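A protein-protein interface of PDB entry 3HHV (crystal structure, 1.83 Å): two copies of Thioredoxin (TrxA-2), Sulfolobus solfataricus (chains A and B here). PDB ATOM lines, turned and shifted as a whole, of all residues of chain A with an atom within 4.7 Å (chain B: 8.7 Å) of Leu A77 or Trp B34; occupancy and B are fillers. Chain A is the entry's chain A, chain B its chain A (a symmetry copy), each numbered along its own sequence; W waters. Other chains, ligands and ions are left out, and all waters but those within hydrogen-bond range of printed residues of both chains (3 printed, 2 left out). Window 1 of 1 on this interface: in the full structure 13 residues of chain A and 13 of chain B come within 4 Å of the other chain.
The side-chain hydroxyl (OG1) of Thr A62 lies within hydrogen-bond range of the indole nitrogen (NE1) of Trp B34, 3.3 Å away. The side-chain amide nitrogen of Gln A66 sits at hydrogen-bond distance from the side-chain carboxylate of Glu B33. OE2 of Glu A63 sits close to OE1 of Glu B33. O of Met A75 sits at hydrogen-bond distance from N of Leu B77 (2.8 Å). N of Leu A77 sits at hydrogen-bond distance from O of Met B75, 2.8 Å away. NE1 of Trp A34 lies within hydrogen-bond range of OG1 of Thr B62 (3.3 Å).
The side-chain amide nitrogen of Gln A66 lies within hydrogen-bond range of the side-chain carboxylate of Glu A63, 2.9 Å away. The backbone carbonyl oxygen (O) of Ser A76 sits at hydrogen-bond distance from the side-chain hydroxyl (OG1) of Thr A79, at 2.5 Å. SG of Cys B35 forms a disulfide with SG of Cys B38 (2.1 Å). N of Thr B62 lies within hydrogen-bond range of O of Trp B31 (2.9 Å). The backbone carbonyl oxygen of Trp A31 is in hydrogen-bond range of the backbone NH of Thr A62, 2.9 Å away. The side-chain sulfur (SG) of Cys A35 forms a disulfide with the side-chain sulfur (SG) of Cys A38, at 2.1 Å.
Among the printed residues, merely in contact across the chains: Trp A34 with Ile B74 (3.2 Å), Ile A74 with Trp B34 (3.2 Å), Met A70 with Trp B34 (3.2 Å), Glu A63 with Glu B63 (3.3 Å), Met A70 with Ala B36 (3.7 Å), Glu A63 with Trp B34 (3.7 Å), Trp A34 with Glu B63 (3.7 Å), Gln A66 with Trp B34 (3.7 Å), Met A75 with Ser B76 (3.7 Å), Ser A76 with Met B75 (3.7 Å), Met A75 with Pro B37 (3.7 Å), Ser A76 with Ser B76 (3.8 Å), Ala A69 with Trp B34 (3.8 Å), Trp A34 with Leu B77 (3.9 Å), Leu A77 with Trp B34 (3.9 Å) and Met A75 with Met B75 (3.98 Å).
Leu A77 touches just these residues of chain B: Trp B34 and Met B75. Trp B34 touches seven residues of chain A. Ser A76 touches two residues of chain B. No residue of chain B comes within 4 Å of Pro A78. Of the printed residues of chain A, Met B75 touches Met A75, Ser A76 and Leu A77. Printed residues of chain B within 4 Å of Glu A63: Glu B33 (3.5 Å), Trp B34 (3.7 Å) and Glu B63 (3.3 Å). Of the printed residues of chain A, Ile B74 touches Trp A34 (3.2 Å). Cys A38 touches none of the printed residues of chain B. The nearest residue of chain B that does not touch Leu A77 is Ser B76 (4.6 Å). The nearest printed residue of chain A that does not touch Trp B34 is Trp A34 (4.04 Å).
Of the 18 printed residues of chain B, 10 touch a printed residue of chain A. Hydrophobic or aromatic side chains of chain B that line the printed part of chain A: Trp B34, Ala B36, Pro B37, Ile B74, Met B75 and Leu B77. Of the 18 printed residues of chain A, 10 touch a printed residue of chain B. Printed residues of chain A that touch a printed residue of chain B: Trp A34, Thr A62, Glu A63, Gln A66, Ala A69, Met A70, Ile A74, Met A75, Ser A76 and Leu A77. Along chain A the printed residues that touch a printed residue of chain B span positions 34 to 77. Among the printed residues, 22 pairs touch across the chains. Among the printed residues, no Asp or Glu carboxylate lies within 4 Å of a Lys or Arg side-chain nitrogen of the other chain.
Trp A34 touches Glu B63, and with the chains exchanged Glu A63 touches Trp B34. Trp A34 touches Ile B74, and with the chains exchanged Ile A74 touches Trp B34. Met B75 touches its own counterpart, Met A75. Met A75 touches Leu B77, and with the chains exchanged Leu A77 touches Met B75. Of the 22 pairs that touch across the chains among the printed residues, 15 have their exchanged pair printed and touching as well.
Water W3 lies within hydrogen-bond range of OD1 of Asn B61 (2.8 Å), N of Glu B33 (2.8 Å) and OE1 of Glu A63 (3.2 Å). Water W2 lies within hydrogen-bond range of the backbone carbonyl oxygen (O) of Ile A74 (2.8 Å), the backbone NH (N) of Ala B36 (2.9 Å) and the backbone carbonyl oxygen (O) of Trp B34 (2.9 Å). Water W1 lies within hydrogen-bond range of O of Ile B74 (2.8 Å) and O of Trp A34 (2.9 Å).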
ATOM      1  N   PHE A  30      24.409  11.724  32.895  1.00  0.00           N
ATOM      2  CA  PHE A  30      25.213  12.159  31.736  1.00  0.00           C
ATOM      3  C   PHE A  30      24.281  12.901  30.791  1.00  0.00           C
ATOM      4  O   PHE A  30      23.262  12.338  30.344  1.00  0.00           O
ATOM      5  CB  PHE A  30      25.841  10.998  30.971  1.00  0.00           C
ATOM      6  CG  PHE A  30      27.017  10.346  31.671  1.00  0.00           C
ATOM      7  CD1 PHE A  30      26.807   9.327  32.598  1.00  0.00           C
ATOM      8  CD2 PHE A  30      28.329  10.760  31.394  1.00  0.00           C
ATOM      9  CE1 PHE A  30      27.907   8.684  33.221  1.00  0.00           C
ATOM     10  CE2 PHE A  30      29.415  10.151  31.980  1.00  0.00           C
ATOM     11  CZ  PHE A  30      29.214   9.107  32.919  1.00  0.00           C
ATOM     12  N   TRP A  31      24.574  14.175  30.576  1.00  0.00           N
ATOM     13  CA  TRP A  31      23.654  15.076  29.859  1.00  0.00           C
ATOM     14  C   TRP A  31      24.412  16.019  28.914  1.00  0.00           C
ATOM     15  O   TRP A  31      25.657  16.058  28.905  1.00  0.00           O
ATOM     16  CB  TRP A  31      22.813  15.877  30.850  1.00  0.00           C
ATOM     17  CG  TRP A  31      23.638  16.934  31.555  1.00  0.00           C
ATOM     18  CD1 TRP A  31      24.585  16.713  32.522  1.00  0.00           C
ATOM     19  CD2 TRP A  31      23.622  18.362  31.325  1.00  0.00           C
ATOM     20  NE1 TRP A  31      25.121  17.908  32.935  1.00  0.00           N
ATOM     21  CE2 TRP A  31      24.567  18.933  32.215  1.00  0.00           C
ATOM     22  CE3 TRP A  31      22.889  19.212  30.474  1.00  0.00           C
ATOM     23  CZ2 TRP A  31      24.817  20.322  32.271  1.00  0.00           C
ATOM     24  CZ3 TRP A  31      23.132  20.615  30.524  1.00  0.00           C
ATOM     25  CH2 TRP A  31      24.091  21.148  31.421  1.00  0.00           C
ATOM     26  N   ALA A  32      23.649  16.732  28.084  1.00  0.00           N
ATOM     27  CA  ALA A  32      24.190  17.746  27.200  1.00  0.00           C
ATOM     28  C   ALA A  32      23.192  18.866  27.059  1.00  0.00           C
ATOM     29  O   ALA A  32      21.970  18.645  27.130  1.00  0.00           O
ATOM     30  CB  ALA A  32      24.559  17.164  25.810  1.00  0.00           C
ATOM     31  N   TRP A  34      22.109  20.589  24.594  1.00  0.00           N
ATOM     32  CA  TRP A  34      21.248  20.547  23.418  1.00  0.00           C
ATOM     33  C   TRP A  34      20.209  19.431  23.470  1.00  0.00           C
ATOM     34  O   TRP A  34      19.426  19.283  22.559  1.00  0.00           O
ATOM     35  CB  TRP A  34      22.122  20.328  22.156  1.00  0.00           C
ATOM     36  CG  TRP A  34      23.103  19.156  22.291  1.00  0.00           C
ATOM     37  CD1 TRP A  34      24.425  19.231  22.603  1.00  0.00           C
ATOM     38  CD2 TRP A  34      22.809  17.764  22.104  1.00  0.00           C
ATOM     39  NE1 TRP A  34      24.973  17.966  22.626  1.00  0.00           N
ATOM     40  CE2 TRP A  34      23.998  17.052  22.339  1.00  0.00           C
ATOM     41  CE3 TRP A  34      21.642  17.044  21.778  1.00  0.00           C
ATOM     42  CZ2 TRP A  34      24.070  15.652  22.219  1.00  0.00           C
ATOM     43  CZ3 TRP A  34      21.711  15.636  21.686  1.00  0.00           C
ATOM     44  CH2 TRP A  34      22.921  14.968  21.907  1.00  0.00           C
ATOM     45  N   CYS A  35      20.242  18.622  24.540  1.00  0.00           N
ATOM     46  CA  CYS A  35      19.444  17.427  24.638  1.00  0.00           C
ATOM     47  C   CYS A  35      18.168  17.726  25.405  1.00  0.00           C
ATOM     48  O   CYS A  35      18.195  17.864  26.647  1.00  0.00           O
ATOM     49  CB  CYS A  35      20.298  16.344  25.342  1.00  0.00           C
ATOM     50  SG  CYS A  35      19.418  14.900  25.904  1.00  0.00           S
ATOM     51  N   CYS A  38      17.204  15.440  28.285  1.00  0.00           N
ATOM     52  CA  CYS A  38      18.171  15.741  29.362  1.00  0.00           C
ATOM     53  C   CYS A  38      17.706  16.897  30.243  1.00  0.00           C
ATOM     54  O   CYS A  38      17.682  16.795  31.482  1.00  0.00           O
ATOM     55  CB  CYS A  38      19.570  16.050  28.780  1.00  0.00           C
ATOM     56  SG  CYS A  38      20.273  14.659  27.816  1.00  0.00           S
ATOM     57  N   THR A  62      28.594  16.112  29.149  1.00  0.00           N
ATOM     58  CA  THR A  62      29.430  15.394  28.190  1.00  0.00           C
ATOM     59  C   THR A  62      30.381  16.306  27.397  1.00  0.00           C
ATOM     60  O   THR A  62      31.497  15.933  27.107  1.00  0.00           O
ATOM     61  CB  THR A  62      28.568  14.589  27.201  1.00  0.00           C
ATOM     62  OG1 THR A  62      27.572  15.448  26.633  1.00  0.00           O
ATOM     63  CG2 THR A  62      27.864  13.408  27.924  1.00  0.00           C
ATOM     64  N   GLU A  63      29.927  17.500  27.057  1.00  0.00           N
ATOM     65  CA  GLU A  63      30.759  18.426  26.301  1.00  0.00           C
ATOM     66  C   GLU A  63      31.900  18.969  27.137  1.00  0.00           C
ATOM     67  O   GLU A  63      32.962  19.292  26.598  1.00  0.00           O
ATOM     68  CB  GLU A  63      29.928  19.565  25.738  1.00  0.00           C
ATOM     69  CG  GLU A  63      30.773  20.509  24.894  1.00  0.00           C
ATOM     70  CD  GLU A  63      31.279  19.838  23.638  1.00  0.00           C
ATOM     71  OE1 GLU A  63      30.608  18.876  23.133  1.00  0.00           O
ATOM     72  OE2 GLU A  63      32.314  20.284  23.129  1.00  0.00           O
ATOM     73  N   GLN A  66      34.685  15.439  28.199  1.00  0.00           N
ATOM     74  CA  GLN A  66      34.599  14.511  27.080  1.00  0.00           C
ATOM     75  C   GLN A  66      35.327  13.200  27.340  1.00  0.00           C
ATOM     76  O   GLN A  66      34.896  12.133  26.852  1.00  0.00           O
ATOM     77  CB  GLN A  66      35.121  15.181  25.800  1.00  0.00           C
ATOM     78  CG  GLN A  66      34.350  16.489  25.448  1.00  0.00           C
ATOM     79  CD  GLN A  66      34.741  17.027  24.080  1.00  0.00           C
ATOM     80  OE1 GLN A  66      35.627  16.481  23.433  1.00  0.00           O
ATOM     81  NE2 GLN A  66      34.102  18.106  23.646  1.00  0.00           N
ATOM     82  N   ALA A  69      32.928  10.904  29.355  1.00  0.00           N
ATOM     83  CA  ALA A  69      31.986  10.458  28.333  1.00  0.00           C
ATOM     84  C   ALA A  69      32.561   9.352  27.443  1.00  0.00           C
ATOM     85  O   ALA A  69      31.933   8.301  27.281  1.00  0.00           O
ATOM     86  CB  ALA A  69      31.461  11.684  27.474  1.00  0.00           C
ATOM     87  N   MET A  70      33.766   9.553  26.925  1.00  0.00           N
ATOM     88  CA  MET A  70      34.343   8.548  26.039  1.00  0.00           C
ATOM     89  C   MET A  70      34.723   7.266  26.746  1.00  0.00           C
ATOM     90  O   MET A  70      34.500   6.166  26.221  1.00  0.00           O
ATOM     91  CB  MET A  70      35.555   9.079  25.292  1.00  0.00           C
ATOM     92  CG  MET A  70      36.154   8.003  24.378  1.00  0.00           C
ATOM     93  SD  MET A  70      36.755   8.749  22.889  1.00  0.00           S
ATOM     94  CE  MET A  70      35.285   9.661  22.496  1.00  0.00           C
ATOM     95  N   ILE A  74      29.651   6.679  26.231  1.00  0.00           N
ATOM     96  CA  ILE A  74      28.361   7.341  26.272  1.00  0.00           C
ATOM     97  C   ILE A  74      27.942   7.684  24.838  1.00  0.00           C
ATOM     98  O   ILE A  74      28.762   8.143  24.060  1.00  0.00           O
ATOM     99  CB  ILE A  74      28.420   8.631  27.123  1.00  0.00           C
ATOM    100  CG1 ILE A  74      28.834   8.295  28.567  1.00  0.00           C
ATOM    101  CG2 ILE A  74      27.065   9.352  27.075  1.00  0.00           C
ATOM    102  CD1 ILE A  74      27.842   7.409  29.343  1.00  0.00           C
ATOM    103  N   MET A  75      26.672   7.446  24.511  1.00  0.00           N
ATOM    104  CA  MET A  75      26.167   7.766  23.164  1.00  0.00           C
ATOM    105  C   MET A  75      24.676   8.126  23.127  1.00  0.00           C
ATOM    106  O   MET A  75      24.237   8.836  22.241  1.00  0.00           O
ATOM    107  CB  MET A  75      26.440   6.596  22.212  1.00  0.00           C
ATOM    108  CG  MET A  75      25.803   5.264  22.635  1.00  0.00           C
ATOM    109  SD  MET A  75      26.529   3.891  21.710  1.00  0.00           S
ATOM    110  CE  MET A  75      27.790   3.360  22.819  1.00  0.00           C
ATOM    111  N   SER A  76      23.912   7.639  24.097  1.00  0.00           N
ATOM    112  CA  SER A  76      22.455   7.771  24.066  1.00  0.00           C
ATOM    113  C   SER A  76      22.063   8.560  25.312  1.00  0.00           C
ATOM    114  O   SER A  76      22.316   8.115  26.444  1.00  0.00           O
ATOM    115  CB  SER A  76      21.833   6.373  24.024  1.00  0.00           C
ATOM    116  OG  SER A  76      20.411   6.409  24.021  1.00  0.00           O
ATOM    117  N   LEU A  77      21.507   9.758  25.106  1.00  0.00           N
ATOM    118  CA  LEU A  77      21.237  10.685  26.221  1.00  0.00           C
ATOM    119  C   LEU A  77      19.742  10.870  26.542  1.00  0.00           C
ATOM    120  O   LEU A  77      18.909  10.736  25.639  1.00  0.00           O
ATOM    121  CB  LEU A  77      21.844  12.053  25.885  1.00  0.00           C
ATOM    122  CG  LEU A  77      23.377  12.106  25.750  1.00  0.00           C
ATOM    123  CD1 LEU A  77      23.804  13.547  25.586  1.00  0.00           C
ATOM    124  CD2 LEU A  77      24.099  11.439  26.928  1.00  0.00           C
ATOM    125  N   PRO A  78      19.404  11.160  27.829  1.00  0.00           N
ATOM    126  CA  PRO A  78      20.347  11.150  28.959  1.00  0.00           C
ATOM    127  C   PRO A  78      20.785   9.707  29.247  1.00  0.00           C
ATOM    128  O   PRO A  78      20.089   8.769  28.873  1.00  0.00           O
ATOM    129  CB  PRO A  78      19.534  11.731  30.128  1.00  0.00           C
ATOM    130  CG  PRO A  78      18.117  11.650  29.725  1.00  0.00           C
ATOM    131  CD  PRO A  78      18.029  11.538  28.232  1.00  0.00           C
ATOM    132  N   THR A  79      21.982   9.540  29.806  1.00  0.00           N
ATOM    133  CA  THR A  79      22.387   8.254  30.345  1.00  0.00           C
ATOM    134  C   THR A  79      22.441   8.429  31.828  1.00  0.00           C
ATOM    135  O   THR A  79      23.198   9.266  32.317  1.00  0.00           O
ATOM    136  CB  THR A  79      23.782   7.823  29.824  1.00  0.00           C
ATOM    137  OG1 THR A  79      23.654   7.501  28.431  1.00  0.00           O
ATOM    138  CG2 THR A  79      24.296   6.567  30.541  1.00  0.00           C
ATOM    139  N   GLY A  94      18.051   7.251  27.805  1.00  0.00           N
ATOM    140  CA  GLY A  94      16.887   8.086  27.432  1.00  0.00           C
ATOM    141  C   GLY A  94      16.058   8.508  28.638  1.00  0.00           C
ATOM    142  O   GLY A  94      16.179   7.927  29.714  1.00  0.00           O
ATOM    143  N   TRP B  31      26.377  14.546  15.268  1.00  0.00           N
ATOM    144  CA  TRP B  31      27.505  13.965  16.018  1.00  0.00           C
ATOM    145  C   TRP B  31      27.966  14.891  17.152  1.00  0.00           C
ATOM    146  O   TRP B  31      27.492  16.037  17.280  1.00  0.00           O
ATOM    147  CB  TRP B  31      28.667  13.656  15.077  1.00  0.00           C
ATOM    148  CG  TRP B  31      29.354  14.921  14.606  1.00  0.00           C
ATOM    149  CD1 TRP B  31      28.856  15.831  13.708  1.00  0.00           C
ATOM    150  CD2 TRP B  31      30.637  15.438  15.032  1.00  0.00           C
ATOM    151  NE1 TRP B  31      29.759  16.846  13.519  1.00  0.00           N
ATOM    152  CE2 TRP B  31      30.851  16.645  14.322  1.00  0.00           C
ATOM    153  CE3 TRP B  31      31.630  14.987  15.924  1.00  0.00           C
ATOM    154  CZ2 TRP B  31      32.016  17.428  14.485  1.00  0.00           C
ATOM    155  CZ3 TRP B  31      32.809  15.768  16.094  1.00  0.00           C
ATOM    156  CH2 TRP B  31      32.984  16.975  15.372  1.00  0.00           C
ATOM    157  N   ALA B  32      28.848  14.363  18.000  1.00  0.00           N
ATOM    158  CA  ALA B  32      29.467  15.129  19.064  1.00  0.00           C
ATOM    159  C   ALA B  32      30.879  14.645  19.269  1.00  0.00           C
ATOM    160  O   ALA B  32      31.184  13.458  19.056  1.00  0.00           O
ATOM    161  CB  ALA B  32      28.661  15.040  20.386  1.00  0.00           C
ATOM    162  N   GLU B  33      31.737  15.557  19.738  1.00  0.00           N
ATOM    163  CA  GLU B  33      33.177  15.296  19.848  1.00  0.00           C
ATOM    164  C   GLU B  33      33.524  14.190  20.841  1.00  0.00           C
ATOM    165  O   GLU B  33      34.559  13.553  20.719  1.00  0.00           O
ATOM    166  CB  GLU B  33      33.908  16.581  20.246  1.00  0.00           C
ATOM    167  CG  GLU B  33      33.881  17.658  19.136  1.00  0.00           C
ATOM    168  CD  GLU B  33      33.958  19.059  19.729  1.00  0.00           C
ATOM    169  OE1 GLU B  33      34.653  19.222  20.771  1.00  0.00           O
ATOM    170  OE2 GLU B  33      33.301  19.984  19.170  1.00  0.00           O
ATOM    171  N   TRP B  34      32.660  13.994  21.842  1.00  0.00           N
ATOM    172  CA  TRP B  34      32.866  13.029  22.917  1.00  0.00           C
ATOM    173  C   TRP B  34      32.281  11.654  22.613  1.00  0.00           C
ATOM    174  O   TRP B  34      32.384  10.756  23.418  1.00  0.00           O
ATOM    175  CB  TRP B  34      32.194  13.560  24.210  1.00  0.00           C
ATOM    176  CG  TRP B  34      30.742  14.007  24.002  1.00  0.00           C
ATOM    177  CD1 TRP B  34      30.298  15.282  23.826  1.00  0.00           C
ATOM    178  CD2 TRP B  34      29.580  13.166  23.964  1.00  0.00           C
ATOM    179  NE1 TRP B  34      28.928  15.284  23.675  1.00  0.00           N
ATOM    180  CE2 TRP B  34      28.470  13.998  23.741  1.00  0.00           C
ATOM    181  CE3 TRP B  34      29.373  11.776  24.076  1.00  0.00           C
ATOM    182  CZ2 TRP B  34      27.158  13.494  23.668  1.00  0.00           C
ATOM    183  CZ3 TRP B  34      28.058  11.271  23.975  1.00  0.00           C
ATOM    184  CH2 TRP B  34      26.977  12.137  23.775  1.00  0.00           C
ATOM    185  N   CYS B  35      31.632  11.516  21.447  1.00  0.00           N
ATOM    186  CA  CYS B  35      30.881  10.333  21.110  1.00  0.00           C
ATOM    187  C   CYS B  35      31.745   9.401  20.278  1.00  0.00           C
ATOM    188  O   CYS B  35      31.972   9.654  19.076  1.00  0.00           O
ATOM    189  CB  CYS B  35      29.613  10.781  20.342  1.00  0.00           C
ATOM    190  SG  CYS B  35      28.713   9.491  19.503  1.00  0.00           S
ATOM    191  N   ALA B  36      32.263   8.341  20.886  1.00  0.00           N
ATOM    192  CA  ALA B  36      33.150   7.419  20.147  1.00  0.00           C
ATOM    193  C   ALA B  36      32.530   6.784  18.851  1.00  0.00           C
ATOM    194  O   ALA B  36      33.168   6.828  17.777  1.00  0.00           O
ATOM    195  CB  ALA B  36      33.735   6.354  21.080  1.00  0.00           C
ATOM    196  N   PRO B  37      31.294   6.231  18.928  1.00  0.00           N
ATOM    197  CA  PRO B  37      30.704   5.704  17.705  1.00  0.00           C
ATOM    198  C   PRO B  37      30.566   6.770  16.620  1.00  0.00           C
ATOM    199  O   PRO B  37      30.639   6.433  15.429  1.00  0.00           O
ATOM    200  CB  PRO B  37      29.309   5.227  18.146  1.00  0.00           C
ATOM    201  CG  PRO B  37      29.404   5.034  19.604  1.00  0.00           C
ATOM    202  CD  PRO B  37      30.396   6.043  20.091  1.00  0.00           C
ATOM    203  N   CYS B  38      30.326   8.029  17.029  1.00  0.00           N
ATOM    204  CA  CYS B  38      30.303   9.177  16.099  1.00  0.00           C
ATOM    205  C   CYS B  38      31.624   9.335  15.351  1.00  0.00           C
ATOM    206  O   CYS B  38      31.654   9.447  14.113  1.00  0.00           O
ATOM    207  CB  CYS B  38      29.959  10.487  16.844  1.00  0.00           C
ATOM    208  SG  CYS B  38      28.321  10.442  17.663  1.00  0.00           S
ATOM    209  N   LEU B  39      32.706   9.325  16.109  1.00  0.00           N
ATOM    210  CA  LEU B  39      34.058   9.545  15.545  1.00  0.00           C
ATOM    211  C   LEU B  39      34.436   8.399  14.621  1.00  0.00           C
ATOM    212  O   LEU B  39      35.063   8.581  13.549  1.00  0.00           O
ATOM    213  CB  LEU B  39      35.051   9.710  16.701  1.00  0.00           C
ATOM    214  CG  LEU B  39      34.790  10.964  17.576  1.00  0.00           C
ATOM    215  CD1 LEU B  39      35.783  11.031  18.737  1.00  0.00           C
ATOM    216  CD2 LEU B  39      34.828  12.271  16.763  1.00  0.00           C
ATOM    217  N   ASN B  61      27.380  19.311  14.192  1.00  0.00           N
ATOM    218  CA  ASN B  61      27.965  19.155  15.529  1.00  0.00           C
ATOM    219  C   ASN B  61      26.950  19.678  16.547  1.00  0.00           C
ATOM    220  O   ASN B  61      26.629  20.883  16.589  1.00  0.00           O
ATOM    221  CB  ASN B  61      29.325  19.898  15.597  1.00  0.00           C
ATOM    222  CG  ASN B  61      30.004  19.816  16.994  1.00  0.00           C
ATOM    223  OD1 ASN B  61      29.368  19.550  18.002  1.00  0.00           O
ATOM    224  ND2 ASN B  61      31.313  20.064  17.028  1.00  0.00           N
ATOM    225  N   THR B  62      26.363  18.760  17.317  1.00  0.00           N
ATOM    226  CA  THR B  62      25.281  19.101  18.237  1.00  0.00           C
ATOM    227  C   THR B  62      25.649  20.213  19.235  1.00  0.00           C
ATOM    228  O   THR B  62      24.828  21.038  19.571  1.00  0.00           O
ATOM    229  CB  THR B  62      24.812  17.862  19.020  1.00  0.00           C
ATOM    230  OG1 THR B  62      25.947  17.215  19.610  1.00  0.00           O
ATOM    231  CG2 THR B  62      24.093  16.858  18.077  1.00  0.00           C
ATOM    232  N   GLU B  63      26.888  20.222  19.696  1.00  0.00           N
ATOM    233  CA  GLU B  63      27.320  21.237  20.648  1.00  0.00           C
ATOM    234  C   GLU B  63      27.423  22.605  20.005  1.00  0.00           C
ATOM    235  O   GLU B  63      27.234  23.622  20.679  1.00  0.00           O
ATOM    236  CB  GLU B  63      28.641  20.853  21.287  1.00  0.00           C
ATOM    237  CG  GLU B  63      29.076  21.872  22.329  1.00  0.00           C
ATOM    238  CD  GLU B  63      28.145  21.891  23.519  1.00  0.00           C
ATOM    239  OE1 GLU B  63      27.500  20.831  23.820  1.00  0.00           O
ATOM    240  OE2 GLU B  63      28.081  22.935  24.179  1.00  0.00           O
ATOM    241  N   GLY B  73      14.927  17.085  18.177  1.00  0.00           N
ATOM    242  CA  GLY B  73      14.795  16.202  19.345  1.00  0.00           C
ATOM    243  C   GLY B  73      15.887  15.153  19.309  1.00  0.00           C
ATOM    244  O   GLY B  73      15.646  13.974  19.602  1.00  0.00           O
ATOM    245  N   ILE B  74      17.097  15.590  18.963  1.00  0.00           N
ATOM    246  CA  ILE B  74      18.229  14.685  18.896  1.00  0.00           C
ATOM    247  C   ILE B  74      18.581  14.238  20.321  1.00  0.00           C
ATOM    248  O   ILE B  74      18.591  15.054  21.227  1.00  0.00           O
ATOM    249  CB  ILE B  74      19.454  15.367  18.244  1.00  0.00           C
ATOM    250  CG1 ILE B  74      19.113  15.814  16.812  1.00  0.00           C
ATOM    251  CG2 ILE B  74      20.658  14.414  18.269  1.00  0.00           C
ATOM    252  CD1 ILE B  74      18.784  14.673  15.831  1.00  0.00           C
ATOM    253  N   MET B  75      18.853  12.945  20.492  1.00  0.00           N
ATOM    254  CA  MET B  75      19.226  12.423  21.819  1.00  0.00           C
ATOM    255  C   MET B  75      20.159  11.206  21.770  1.00  0.00           C
ATOM    256  O   MET B  75      20.902  10.962  22.702  1.00  0.00           O
ATOM    257  CB  MET B  75      17.964  12.075  22.618  1.00  0.00           C
ATOM    258  CG  MET B  75      17.054  11.031  21.956  1.00  0.00           C
ATOM    259  SD  MET B  75      15.426  11.019  22.741  1.00  0.00           S
ATOM    260  CE  MET B  75      14.530  12.111  21.688  1.00  0.00           C
ATOM    261  N   SER B  76      20.117  10.456  20.675  1.00  0.00           N
ATOM    262  CA  SER B  76      20.829   9.180  20.591  1.00  0.00           C
ATOM    263  C   SER B  76      21.821   9.311  19.437  1.00  0.00           C
ATOM    264  O   SER B  76      21.417   9.524  18.282  1.00  0.00           O
ATOM    265  CB  SER B  76      19.810   8.058  20.379  1.00  0.00           C
ATOM    266  OG  SER B  76      20.423   6.781  20.256  1.00  0.00           O
ATOM    267  N   LEU B  77      23.117   9.249  19.758  1.00  0.00           N
ATOM    268  CA  LEU B  77      24.171   9.527  18.764  1.00  0.00           C
ATOM    269  C   LEU B  77      24.979   8.287  18.338  1.00  0.00           C
ATOM    270  O   LEU B  77      25.115   7.350  19.132  1.00  0.00           O
ATOM    271  CB  LEU B  77      25.135  10.570  19.344  1.00  0.00           C
ATOM    272  CG  LEU B  77      24.545  11.963  19.625  1.00  0.00           C
ATOM    273  CD1 LEU B  77      25.664  12.897  20.029  1.00  0.00           C
ATOM    274  CD2 LEU B  77      23.751  12.522  18.436  1.00  0.00           C
ATOM    275  N   PRO B  78      25.499   8.275  17.078  1.00  0.00           N
ATOM    276  CA  PRO B  78      25.208   9.287  16.049  1.00  0.00           C
ATOM    277  C   PRO B  78      23.745   9.156  15.602  1.00  0.00           C
ATOM    278  O   PRO B  78      23.143   8.102  15.775  1.00  0.00           O
ATOM    279  CB  PRO B  78      26.175   8.942  14.904  1.00  0.00           C
ATOM    280  CG  PRO B  78      26.643   7.567  15.160  1.00  0.00           C
ATOM    281  CD  PRO B  78      26.441   7.233  16.609  1.00  0.00           C
HETATM  282  O   HOH W   1      17.241  17.440  21.874  1.00  0.00           O
HETATM  283  O   HOH W   2      31.539   7.949  23.635  1.00  0.00           O
HETATM  284  O   HOH W   3      30.724  18.193  20.044  1.00  0.00           O
